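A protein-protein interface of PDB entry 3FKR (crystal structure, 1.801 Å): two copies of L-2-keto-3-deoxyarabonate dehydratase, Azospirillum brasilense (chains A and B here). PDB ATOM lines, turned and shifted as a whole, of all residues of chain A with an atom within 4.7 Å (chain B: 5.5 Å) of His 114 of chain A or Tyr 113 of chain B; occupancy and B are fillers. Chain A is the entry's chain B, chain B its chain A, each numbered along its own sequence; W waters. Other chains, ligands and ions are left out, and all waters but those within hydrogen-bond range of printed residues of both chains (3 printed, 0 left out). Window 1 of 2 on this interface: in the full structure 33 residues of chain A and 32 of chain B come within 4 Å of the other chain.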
ATOM      1  N   TYR A  87      30.025  25.364 -28.262  1.00  0.00           N
ATOM      2  CA  TYR A  87      31.085  24.422 -28.666  1.00  0.00           C
ATOM      3  C   TYR A  87      32.041  25.113 -29.664  1.00  0.00           C
ATOM      4  O   TYR A  87      33.270  25.051 -29.479  1.00  0.00           O
ATOM      5  CB  TYR A  87      30.448  23.167 -29.266  1.00  0.00           C
ATOM      6  CG  TYR A  87      31.495  22.154 -29.717  1.00  0.00           C
ATOM      7  CD1 TYR A  87      32.171  22.310 -30.927  1.00  0.00           C
ATOM      8  CD2 TYR A  87      31.804  21.061 -28.913  1.00  0.00           C
ATOM      9  CE1 TYR A  87      33.182  21.369 -31.313  1.00  0.00           C
ATOM     10  CE2 TYR A  87      32.816  20.136 -29.285  1.00  0.00           C
ATOM     11  CZ  TYR A  87      33.462  20.292 -30.508  1.00  0.00           C
ATOM     12  OH  TYR A  87      34.417  19.340 -30.804  1.00  0.00           O
ATOM     13  N   TYR A 113      32.255  21.710 -25.117  1.00  0.00           N
ATOM     14  CA  TYR A 113      32.024  20.265 -24.989  1.00  0.00           C
ATOM     15  C   TYR A 113      30.605  20.120 -25.560  1.00  0.00           C
ATOM     16  O   TYR A 113      29.925  21.126 -25.813  1.00  0.00           O
ATOM     17  CB  TYR A 113      32.033  19.869 -23.501  1.00  0.00           C
ATOM     18  CG  TYR A 113      30.774  20.383 -22.838  1.00  0.00           C
ATOM     19  CD1 TYR A 113      29.650  19.571 -22.748  1.00  0.00           C
ATOM     20  CD2 TYR A 113      30.725  21.688 -22.299  1.00  0.00           C
ATOM     21  CE1 TYR A 113      28.489  20.044 -22.212  1.00  0.00           C
ATOM     22  CE2 TYR A 113      29.551  22.169 -21.716  1.00  0.00           C
ATOM     23  CZ  TYR A 113      28.442  21.345 -21.717  1.00  0.00           C
ATOM     24  OH  TYR A 113      27.310  21.783 -21.115  1.00  0.00           O
ATOM     25  N   HIS A 114      30.118  18.907 -25.749  1.00  0.00           N
ATOM     26  CA  HIS A 114      28.688  18.692 -25.995  1.00  0.00           C
ATOM     27  C   HIS A 114      28.203  17.425 -25.402  1.00  0.00           C
ATOM     28  O   HIS A 114      28.847  16.362 -25.498  1.00  0.00           O
ATOM     29  CB  HIS A 114      28.253  18.700 -27.522  1.00  0.00           C
ATOM     30  CG  HIS A 114      26.757  18.488 -27.719  1.00  0.00           C
ATOM     31  ND1 HIS A 114      26.206  17.322 -28.224  1.00  0.00           N
ATOM     32  CD2 HIS A 114      25.700  19.307 -27.457  1.00  0.00           C
ATOM     33  CE1 HIS A 114      24.883  17.415 -28.229  1.00  0.00           C
ATOM     34  NE2 HIS A 114      24.548  18.621 -27.789  1.00  0.00           N
ATOM     35  N   GLY A 115      27.052  17.492 -24.739  1.00  0.00           N
ATOM     36  CA  GLY A 115      26.454  16.314 -24.169  1.00  0.00           C
ATOM     37  C   GLY A 115      27.370  15.644 -23.154  1.00  0.00           C
ATOM     38  O   GLY A 115      28.267  16.273 -22.565  1.00  0.00           O
ATOM     39  N   ALA A 116      27.165  14.357 -22.955  1.00  0.00           N
ATOM     40  CA  ALA A 116      28.051  13.556 -22.046  1.00  0.00           C
ATOM     41  C   ALA A 116      29.291  12.997 -22.734  1.00  0.00           C
ATOM     42  O   ALA A 116      30.191  12.495 -22.086  1.00  0.00           O
ATOM     43  CB  ALA A 116      27.265  12.366 -21.415  1.00  0.00           C
ATOM     44  N   THR A 117      29.314  13.066 -24.064  1.00  0.00           N
ATOM     45  CA  THR A 117      30.319  12.314 -24.830  1.00  0.00           C
ATOM     46  C   THR A 117      31.379  13.173 -25.534  1.00  0.00           C
ATOM     47  O   THR A 117      32.555  12.795 -25.618  1.00  0.00           O
ATOM     48  CB  THR A 117      29.657  11.375 -25.895  1.00  0.00           C
ATOM     49  OG1 THR A 117      28.573  10.643 -25.321  1.00  0.00           O
ATOM     50  CG2 THR A 117      30.654  10.367 -26.396  1.00  0.00           C
ATOM     51  N   PHE A 118      30.976  14.320 -26.071  1.00  0.00           N
ATOM     52  CA  PHE A 118      31.860  15.058 -26.921  1.00  0.00           C
ATOM     53  C   PHE A 118      32.752  15.993 -26.086  1.00  0.00           C
ATOM     54  O   PHE A 118      32.264  16.900 -25.407  1.00  0.00           O
ATOM     55  CB  PHE A 118      31.088  15.800 -28.043  1.00  0.00           C
ATOM     56  CG  PHE A 118      30.271  14.877 -28.934  1.00  0.00           C
ATOM     57  CD1 PHE A 118      30.890  14.177 -30.002  1.00  0.00           C
ATOM     58  CD2 PHE A 118      28.910  14.674 -28.691  1.00  0.00           C
ATOM     59  CE1 PHE A 118      30.176  13.327 -30.803  1.00  0.00           C
ATOM     60  CE2 PHE A 118      28.159  13.813 -29.483  1.00  0.00           C
ATOM     61  CZ  PHE A 118      28.803  13.118 -30.560  1.00  0.00           C
ATOM     62  N   ARG A 119      34.052  15.761 -26.121  1.00  0.00           N
ATOM     63  CA  ARG A 119      35.012  16.648 -25.429  1.00  0.00           C
ATOM     64  C   ARG A 119      36.140  17.050 -26.367  1.00  0.00           C
ATOM     65  O   ARG A 119      36.238  16.508 -27.452  1.00  0.00           O
ATOM     66  CB  ARG A 119      35.663  15.953 -24.249  1.00  0.00           C
ATOM     67  CG  ARG A 119      35.175  16.369 -22.894  1.00  0.00           C
ATOM     68  CD  ARG A 119      33.739  16.113 -22.850  1.00  0.00           C
ATOM     69  NE  ARG A 119      33.356  15.225 -21.772  1.00  0.00           N
ATOM     70  CZ  ARG A 119      32.105  15.179 -21.340  1.00  0.00           C
ATOM     71  NH1 ARG A 119      31.730  14.360 -20.365  1.00  0.00           N
ATOM     72  NH2 ARG A 119      31.235  15.986 -21.893  1.00  0.00           N
ATOM     73  N   ASN B  51      24.428  14.031 -34.691  1.00  0.00           N
ATOM     74  CA  ASN B  51      25.673  14.391 -34.035  1.00  0.00           C
ATOM     75  C   ASN B  51      26.826  14.037 -34.980  1.00  0.00           C
ATOM     76  O   ASN B  51      27.820  14.763 -34.968  1.00  0.00           O
ATOM     77  CB  ASN B  51      25.819  13.880 -32.550  1.00  0.00           C
ATOM     78  CG  ASN B  51      24.827  14.597 -31.491  1.00  0.00           C
ATOM     79  OD1 ASN B  51      24.187  13.874 -30.709  1.00  0.00           O
ATOM     80  ND2 ASN B  51      24.784  15.981 -31.400  1.00  0.00           N
ATOM     81  N   GLN B  55      26.289  18.674 -35.529  1.00  0.00           N
ATOM     82  CA  GLN B  55      25.213  19.638 -35.225  1.00  0.00           C
ATOM     83  C   GLN B  55      25.500  20.525 -33.991  1.00  0.00           C
ATOM     84  O   GLN B  55      25.095  21.670 -33.964  1.00  0.00           O
ATOM     85  CB  GLN B  55      23.890  18.916 -35.126  1.00  0.00           C
ATOM     86  CG  GLN B  55      23.758  18.150 -33.898  1.00  0.00           C
ATOM     87  CD  GLN B  55      23.341  19.066 -32.734  1.00  0.00           C
ATOM     88  OE1 GLN B  55      22.776  20.159 -32.914  1.00  0.00           O
ATOM     89  NE2 GLN B  55      23.635  18.635 -31.563  1.00  0.00           N
ATOM     90  N   PHE B  56      26.277  20.033 -33.052  1.00  0.00           N
ATOM     91  CA  PHE B  56      26.693  20.821 -31.867  1.00  0.00           C
ATOM     92  C   PHE B  56      27.610  21.983 -32.167  1.00  0.00           C
ATOM     93  O   PHE B  56      27.755  22.874 -31.340  1.00  0.00           O
ATOM     94  CB  PHE B  56      27.364  19.879 -30.808  1.00  0.00           C
ATOM     95  CG  PHE B  56      28.403  18.964 -31.398  1.00  0.00           C
ATOM     96  CD1 PHE B  56      28.050  17.713 -31.817  1.00  0.00           C
ATOM     97  CD2 PHE B  56      29.726  19.407 -31.580  1.00  0.00           C
ATOM     98  CE1 PHE B  56      29.016  16.867 -32.378  1.00  0.00           C
ATOM     99  CE2 PHE B  56      30.704  18.566 -32.125  1.00  0.00           C
ATOM    100  CZ  PHE B  56      30.340  17.303 -32.533  1.00  0.00           C
ATOM    101  N   TYR B  87      16.406  20.405 -25.601  1.00  0.00           N
ATOM    102  CA  TYR B  87      15.865  20.205 -24.211  1.00  0.00           C
ATOM    103  C   TYR B  87      14.432  20.667 -24.095  1.00  0.00           C
ATOM    104  O   TYR B  87      13.590  19.928 -23.599  1.00  0.00           O
ATOM    105  CB  TYR B  87      16.762  20.929 -23.207  1.00  0.00           C
ATOM    106  CG  TYR B  87      16.337  20.736 -21.756  1.00  0.00           C
ATOM    107  CD1 TYR B  87      15.241  21.421 -21.245  1.00  0.00           C
ATOM    108  CD2 TYR B  87      17.019  19.821 -20.922  1.00  0.00           C
ATOM    109  CE1 TYR B  87      14.825  21.237 -19.898  1.00  0.00           C
ATOM    110  CE2 TYR B  87      16.613  19.611 -19.568  1.00  0.00           C
ATOM    111  CZ  TYR B  87      15.529  20.336 -19.076  1.00  0.00           C
ATOM    112  OH  TYR B  87      15.157  20.125 -17.740  1.00  0.00           O
ATOM    113  N   MET B 110      16.910  12.845 -29.601  1.00  0.00           N
ATOM    114  CA  MET B 110      17.380  12.366 -28.318  1.00  0.00           C
ATOM    115  C   MET B 110      16.354  12.757 -27.242  1.00  0.00           C
ATOM    116  O   MET B 110      15.569  13.711 -27.422  1.00  0.00           O
ATOM    117  CB  MET B 110      18.659  13.081 -27.914  1.00  0.00           C
ATOM    118  CG  MET B 110      19.808  12.898 -28.816  1.00  0.00           C
ATOM    119  SD  MET B 110      20.606  11.437 -28.133  1.00  0.00           S
ATOM    120  CE  MET B 110      22.185  12.051 -27.921  1.00  0.00           C
ATOM    121  N   PRO B 111      16.399  12.064 -26.102  1.00  0.00           N
ATOM    122  CA  PRO B 111      15.570  12.552 -24.992  1.00  0.00           C
ATOM    123  C   PRO B 111      16.160  13.894 -24.530  1.00  0.00           C
ATOM    124  O   PRO B 111      17.335  14.188 -24.740  1.00  0.00           O
ATOM    125  CB  PRO B 111      15.784  11.449 -23.889  1.00  0.00           C
ATOM    126  CG  PRO B 111      17.232  10.931 -24.155  1.00  0.00           C
ATOM    127  CD  PRO B 111      17.274  10.922 -25.737  1.00  0.00           C
ATOM    128  N   PRO B 112      15.303  14.718 -23.884  1.00  0.00           N
ATOM    129  CA  PRO B 112      15.724  15.997 -23.407  1.00  0.00           C
ATOM    130  C   PRO B 112      16.813  15.795 -22.363  1.00  0.00           C
ATOM    131  O   PRO B 112      16.584  14.959 -21.489  1.00  0.00           O
ATOM    132  CB  PRO B 112      14.423  16.590 -22.794  1.00  0.00           C
ATOM    133  CG  PRO B 112      13.516  15.364 -22.517  1.00  0.00           C
ATOM    134  CD  PRO B 112      13.878  14.430 -23.678  1.00  0.00           C
ATOM    135  N   TYR B 113      17.918  16.545 -22.451  1.00  0.00           N
ATOM    136  CA  TYR B 113      18.981  16.523 -21.456  1.00  0.00           C
ATOM    137  C   TYR B 113      19.827  17.703 -21.761  1.00  0.00           C
ATOM    138  O   TYR B 113      19.653  18.345 -22.839  1.00  0.00           O
ATOM    139  CB  TYR B 113      19.873  15.243 -21.590  1.00  0.00           C
ATOM    140  CG  TYR B 113      20.780  15.315 -22.795  1.00  0.00           C
ATOM    141  CD1 TYR B 113      22.078  15.781 -22.650  1.00  0.00           C
ATOM    142  CD2 TYR B 113      20.306  14.940 -24.073  1.00  0.00           C
ATOM    143  CE1 TYR B 113      22.891  15.889 -23.694  1.00  0.00           C
ATOM    144  CE2 TYR B 113      21.123  15.035 -25.171  1.00  0.00           C
ATOM    145  CZ  TYR B 113      22.433  15.545 -24.948  1.00  0.00           C
ATOM    146  OH  TYR B 113      23.318  15.685 -25.954  1.00  0.00           O
ATOM    147  N   HIS B 114      20.732  18.039 -20.865  1.00  0.00           N
ATOM    148  CA  HIS B 114      21.767  19.016 -21.235  1.00  0.00           C
ATOM    149  C   HIS B 114      23.069  18.728 -20.601  1.00  0.00           C
ATOM    150  O   HIS B 114      23.169  18.505 -19.389  1.00  0.00           O
ATOM    151  CB  HIS B 114      21.394  20.502 -20.911  1.00  0.00           C
ATOM    152  CG  HIS B 114      22.454  21.477 -21.411  1.00  0.00           C
ATOM    153  ND1 HIS B 114      23.408  22.059 -20.589  1.00  0.00           N
ATOM    154  CD2 HIS B 114      22.735  21.903 -22.672  1.00  0.00           C
ATOM    155  CE1 HIS B 114      24.233  22.809 -21.326  1.00  0.00           C
ATOM    156  NE2 HIS B 114      23.841  22.726 -22.594  1.00  0.00           N
ATOM    157  N   GLY B 115      24.128  18.754 -21.389  1.00  0.00           N
ATOM    158  CA  GLY B 115      25.416  18.423 -20.824  1.00  0.00           C
ATOM    159  C   GLY B 115      25.523  17.086 -20.093  1.00  0.00           C
ATOM    160  O   GLY B 115      24.785  16.125 -20.364  1.00  0.00           O
ATOM    161  N   PHE B 118      22.306  17.649 -16.581  1.00  0.00           N
ATOM    162  CA  PHE B 118      20.892  18.016 -16.520  1.00  0.00           C
ATOM    163  C   PHE B 118      20.106  16.877 -17.161  1.00  0.00           C
ATOM    164  O   PHE B 118      20.274  16.609 -18.332  1.00  0.00           O
ATOM    165  CB  PHE B 118      20.646  19.413 -17.147  1.00  0.00           C
ATOM    166  CG  PHE B 118      21.366  20.524 -16.425  1.00  0.00           C
ATOM    167  CD1 PHE B 118      20.796  21.119 -15.297  1.00  0.00           C
ATOM    168  CD2 PHE B 118      22.636  20.937 -16.835  1.00  0.00           C
ATOM    169  CE1 PHE B 118      21.470  22.085 -14.616  1.00  0.00           C
ATOM    170  CE2 PHE B 118      23.322  21.932 -16.169  1.00  0.00           C
ATOM    171  CZ  PHE B 118      22.752  22.516 -15.050  1.00  0.00           C
ATOM    172  N   ARG B 119      19.353  16.121 -16.361  1.00  0.00           N
ATOM    173  CA  ARG B 119      18.478  15.088 -16.914  1.00  0.00           C
ATOM    174  C   ARG B 119      17.054  15.327 -16.490  1.00  0.00           C
ATOM    175  O   ARG B 119      16.762  16.194 -15.614  1.00  0.00           O
ATOM    176  CB  ARG B 119      18.865  13.683 -16.425  1.00  0.00           C
ATOM    177  CG  ARG B 119      20.370  13.377 -16.329  1.00  0.00           C
ATOM    178  CD  ARG B 119      20.851  12.487 -17.482  1.00  0.00           C
ATOM    179  NE  ARG B 119      22.301  12.283 -17.493  1.00  0.00           N
ATOM    180  CZ  ARG B 119      23.176  12.928 -18.274  1.00  0.00           C
ATOM    181  NH1 ARG B 119      24.470  12.631 -18.192  1.00  0.00           N
ATOM    182  NH2 ARG B 119      22.789  13.868 -19.129  1.00  0.00           N
ATOM    183  N   VAL B 120      16.170  14.532 -17.071  1.00  0.00           N
ATOM    184  CA  VAL B 120      14.767  14.678 -16.905  1.00  0.00           C
ATOM    185  C   VAL B 120      14.214  13.301 -16.489  1.00  0.00           C
ATOM    186  O   VAL B 120      14.606  12.273 -17.038  1.00  0.00           O
ATOM    187  CB  VAL B 120      14.230  15.052 -18.355  1.00  0.00           C
ATOM    188  CG1 VAL B 120      12.790  15.142 -18.392  1.00  0.00           C
ATOM    189  CG2 VAL B 120      14.909  16.387 -18.907  1.00  0.00           C
ATOM    190  N   ALA B 147      25.520   9.893 -25.678  1.00  0.00           N
ATOM    191  CA  ALA B 147      25.677  11.326 -25.535  1.00  0.00           C
ATOM    192  C   ALA B 147      24.619  11.989 -24.627  1.00  0.00           C
ATOM    193  O   ALA B 147      24.909  13.028 -24.014  1.00  0.00           O
ATOM    194  CB  ALA B 147      25.698  11.996 -26.944  1.00  0.00           C
ATOM    195  N   SER B 148      23.429  11.414 -24.530  1.00  0.00           N
ATOM    196  CA  SER B 148      22.428  12.036 -23.646  1.00  0.00           C
ATOM    197  C   SER B 148      22.633  11.730 -22.163  1.00  0.00           C
ATOM    198  O   SER B 148      21.984  12.365 -21.295  1.00  0.00           O
ATOM    199  CB  SER B 148      21.026  11.568 -24.036  1.00  0.00           C
ATOM    200  OG  SER B 148      20.950  10.150 -23.847  1.00  0.00           O
ATOM    201  N   GLY B 149      23.485  10.743 -21.864  1.00  0.00           N
ATOM    202  CA  GLY B 149      23.656  10.226 -20.510  1.00  0.00           C
ATOM    203  C   GLY B 149      22.369   9.811 -19.818  1.00  0.00           C
ATOM    204  O   GLY B 149      22.299   9.807 -18.576  1.00  0.00           O
ATOM    205  N   THR B 150      21.365   9.421 -20.597  1.00  0.00           N
ATOM    206  CA  THR B 150      20.000   9.247 -20.125  1.00  0.00           C
ATOM    207  C   THR B 150      19.634   7.819 -20.429  1.00  0.00           C
ATOM    208  O   THR B 150      19.801   7.355 -21.539  1.00  0.00           O
ATOM    209  CB  THR B 150      19.032  10.238 -20.861  1.00  0.00           C
ATOM    210  OG1 THR B 150      19.367  11.567 -20.454  1.00  0.00           O
ATOM    211  CG2 THR B 150      17.542   9.940 -20.561  1.00  0.00           C
HETATM  212  O   HOH W   1      27.385  24.176 -28.625  1.00  0.00           O
HETATM  213  O   HOH W   2      25.024  19.348 -24.009  1.00  0.00           O
HETATM  214  O   HOH W   3      22.669  20.626 -29.540  1.00  0.00           O
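Water W2 lies within hydrogen-bond range of the backbone NH (N) of Gly 115 of chain B and the backbone NH (N) of Gly 115 of chain A. Water W1 bridges the backbone NH (N) of Tyr 87 of chain A and the backbone carbonyl oxygen (O) of Phe 56 of chain B. Water W3 lies within hydrogen-bond range of the side-chain amide nitrogen of Gln 55 of chain B (3.0 Å) and a ring nitrogen (NE2) of His 114 of chain A (3.3 Å).
Printed residues of chain B within 4 Å of His 114 of chain A: Asn 51 (3.5 Å), Gln 55 (3.8 Å), Phe 56 (3.4 Å) and Tyr 113 (3.3 Å). Of chain A, only His 114 (3.3 Å) and Gly 115 (3.6 Å) come within 4 Å of Tyr 113 of chain B. Of the printed residues of chain A, Ala 147 of chain B touches Gly 115 (3.6 Å), Ala 116 (2.8 Å), Thr 117 (3.0 Å) and Phe 118 (3.98 Å). Of the printed residues of chain B, Ala 116 of chain A touches Gly 115 and Ala 147. Printed residues of chain B within 4 Å of Tyr 113 of chain A: His 114 (3.3 Å) and Gly 115 (3.7 Å). Printed residues of chain A within 4 Å of Phe 56 of chain B: Tyr 87 and His 114. The nearest residue of chain A that does not touch Tyr 113 of chain B is Ala 116 of chain A (4.6 Å). The nearest printed residue of chain A that does not touch Gln 55 of chain B is Phe 118 of chain A (6.9 Å).
Hydrophobic or aromatic side chains of chain B that line the printed part of chain A: Phe 56, Tyr 113, His 114 and Ala 147. Among the printed residues, 15 pairs touch across the chains. Among the printed residues, no Asp or Glu carboxylate lies within 4 Å of a Lys or Arg side-chain nitrogen of the other chain.
Tyr 113 of chain A touches His 114 of chain B, and with the chains exchanged His 114 of chain A touches Tyr 113 of chain B. Tyr 113 of chain A touches Gly 115 of chain B, and with the chains exchanged Gly 115 of chain A touches Tyr 113 of chain B. Gly 115 of chain A touches its own counterpart, Gly 115 of chain B. 6 positions are printed for both chains.
The side-chain amide nitrogen (ND2) of Asn 51 of chain B lies close to the side-chain amide nitrogen (NE2) of Gln 55 of chain B, at 2.9 Å. The backbone carbonyl oxygen of Gly 115 of chain B is in hydrogen-bond range of the guanidinium group of Arg 119 of chain B, at 3.3 Å. The backbone carbonyl oxygen of Gly 115 of chain A lies within hydrogen-bond range of the guanidinium group of Arg 119 of chain A (3.1 Å). NH1 of Arg 119 of chain A is in hydrogen-bond range of O of Ala 116 of chain A (3.0 Å).
N of Ala 116 of chain A sits at hydrogen-bond distance from O of Ala 147 of chain B (2.8 Å). The backbone NH (N) of Ala 147 of chain B sits close to the side-chain hydroxyl (OG1) of Thr 117 of chain A, 3.2 Å away.
Among the printed residues, merely in contact across the chains: Tyr 113 of chain A with His 114 of chain B, His 114 of chain A with Tyr 113 of chain B, Tyr 87 of chain A with Phe 56 of chain B, His 114 of chain A with Phe 56 of chain B, His 114 of chain A with Asn 51 of chain B, Gly 115 of chain A with Tyr 113 of chain B, Gly 115 of chain A with Ala 147 of chain B, Phe 118 of chain A with Asn 51 of chain B, Tyr 113 of chain A with Gly 115 of chain B, His 114 of chain A with Gln 55 of chain B, Gly 115 of chain A with Gly 115 of chain B, Ala 116 of chain A with Gly 115 of chain B and Phe 118 of chain A with Ala 147 of chain B.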
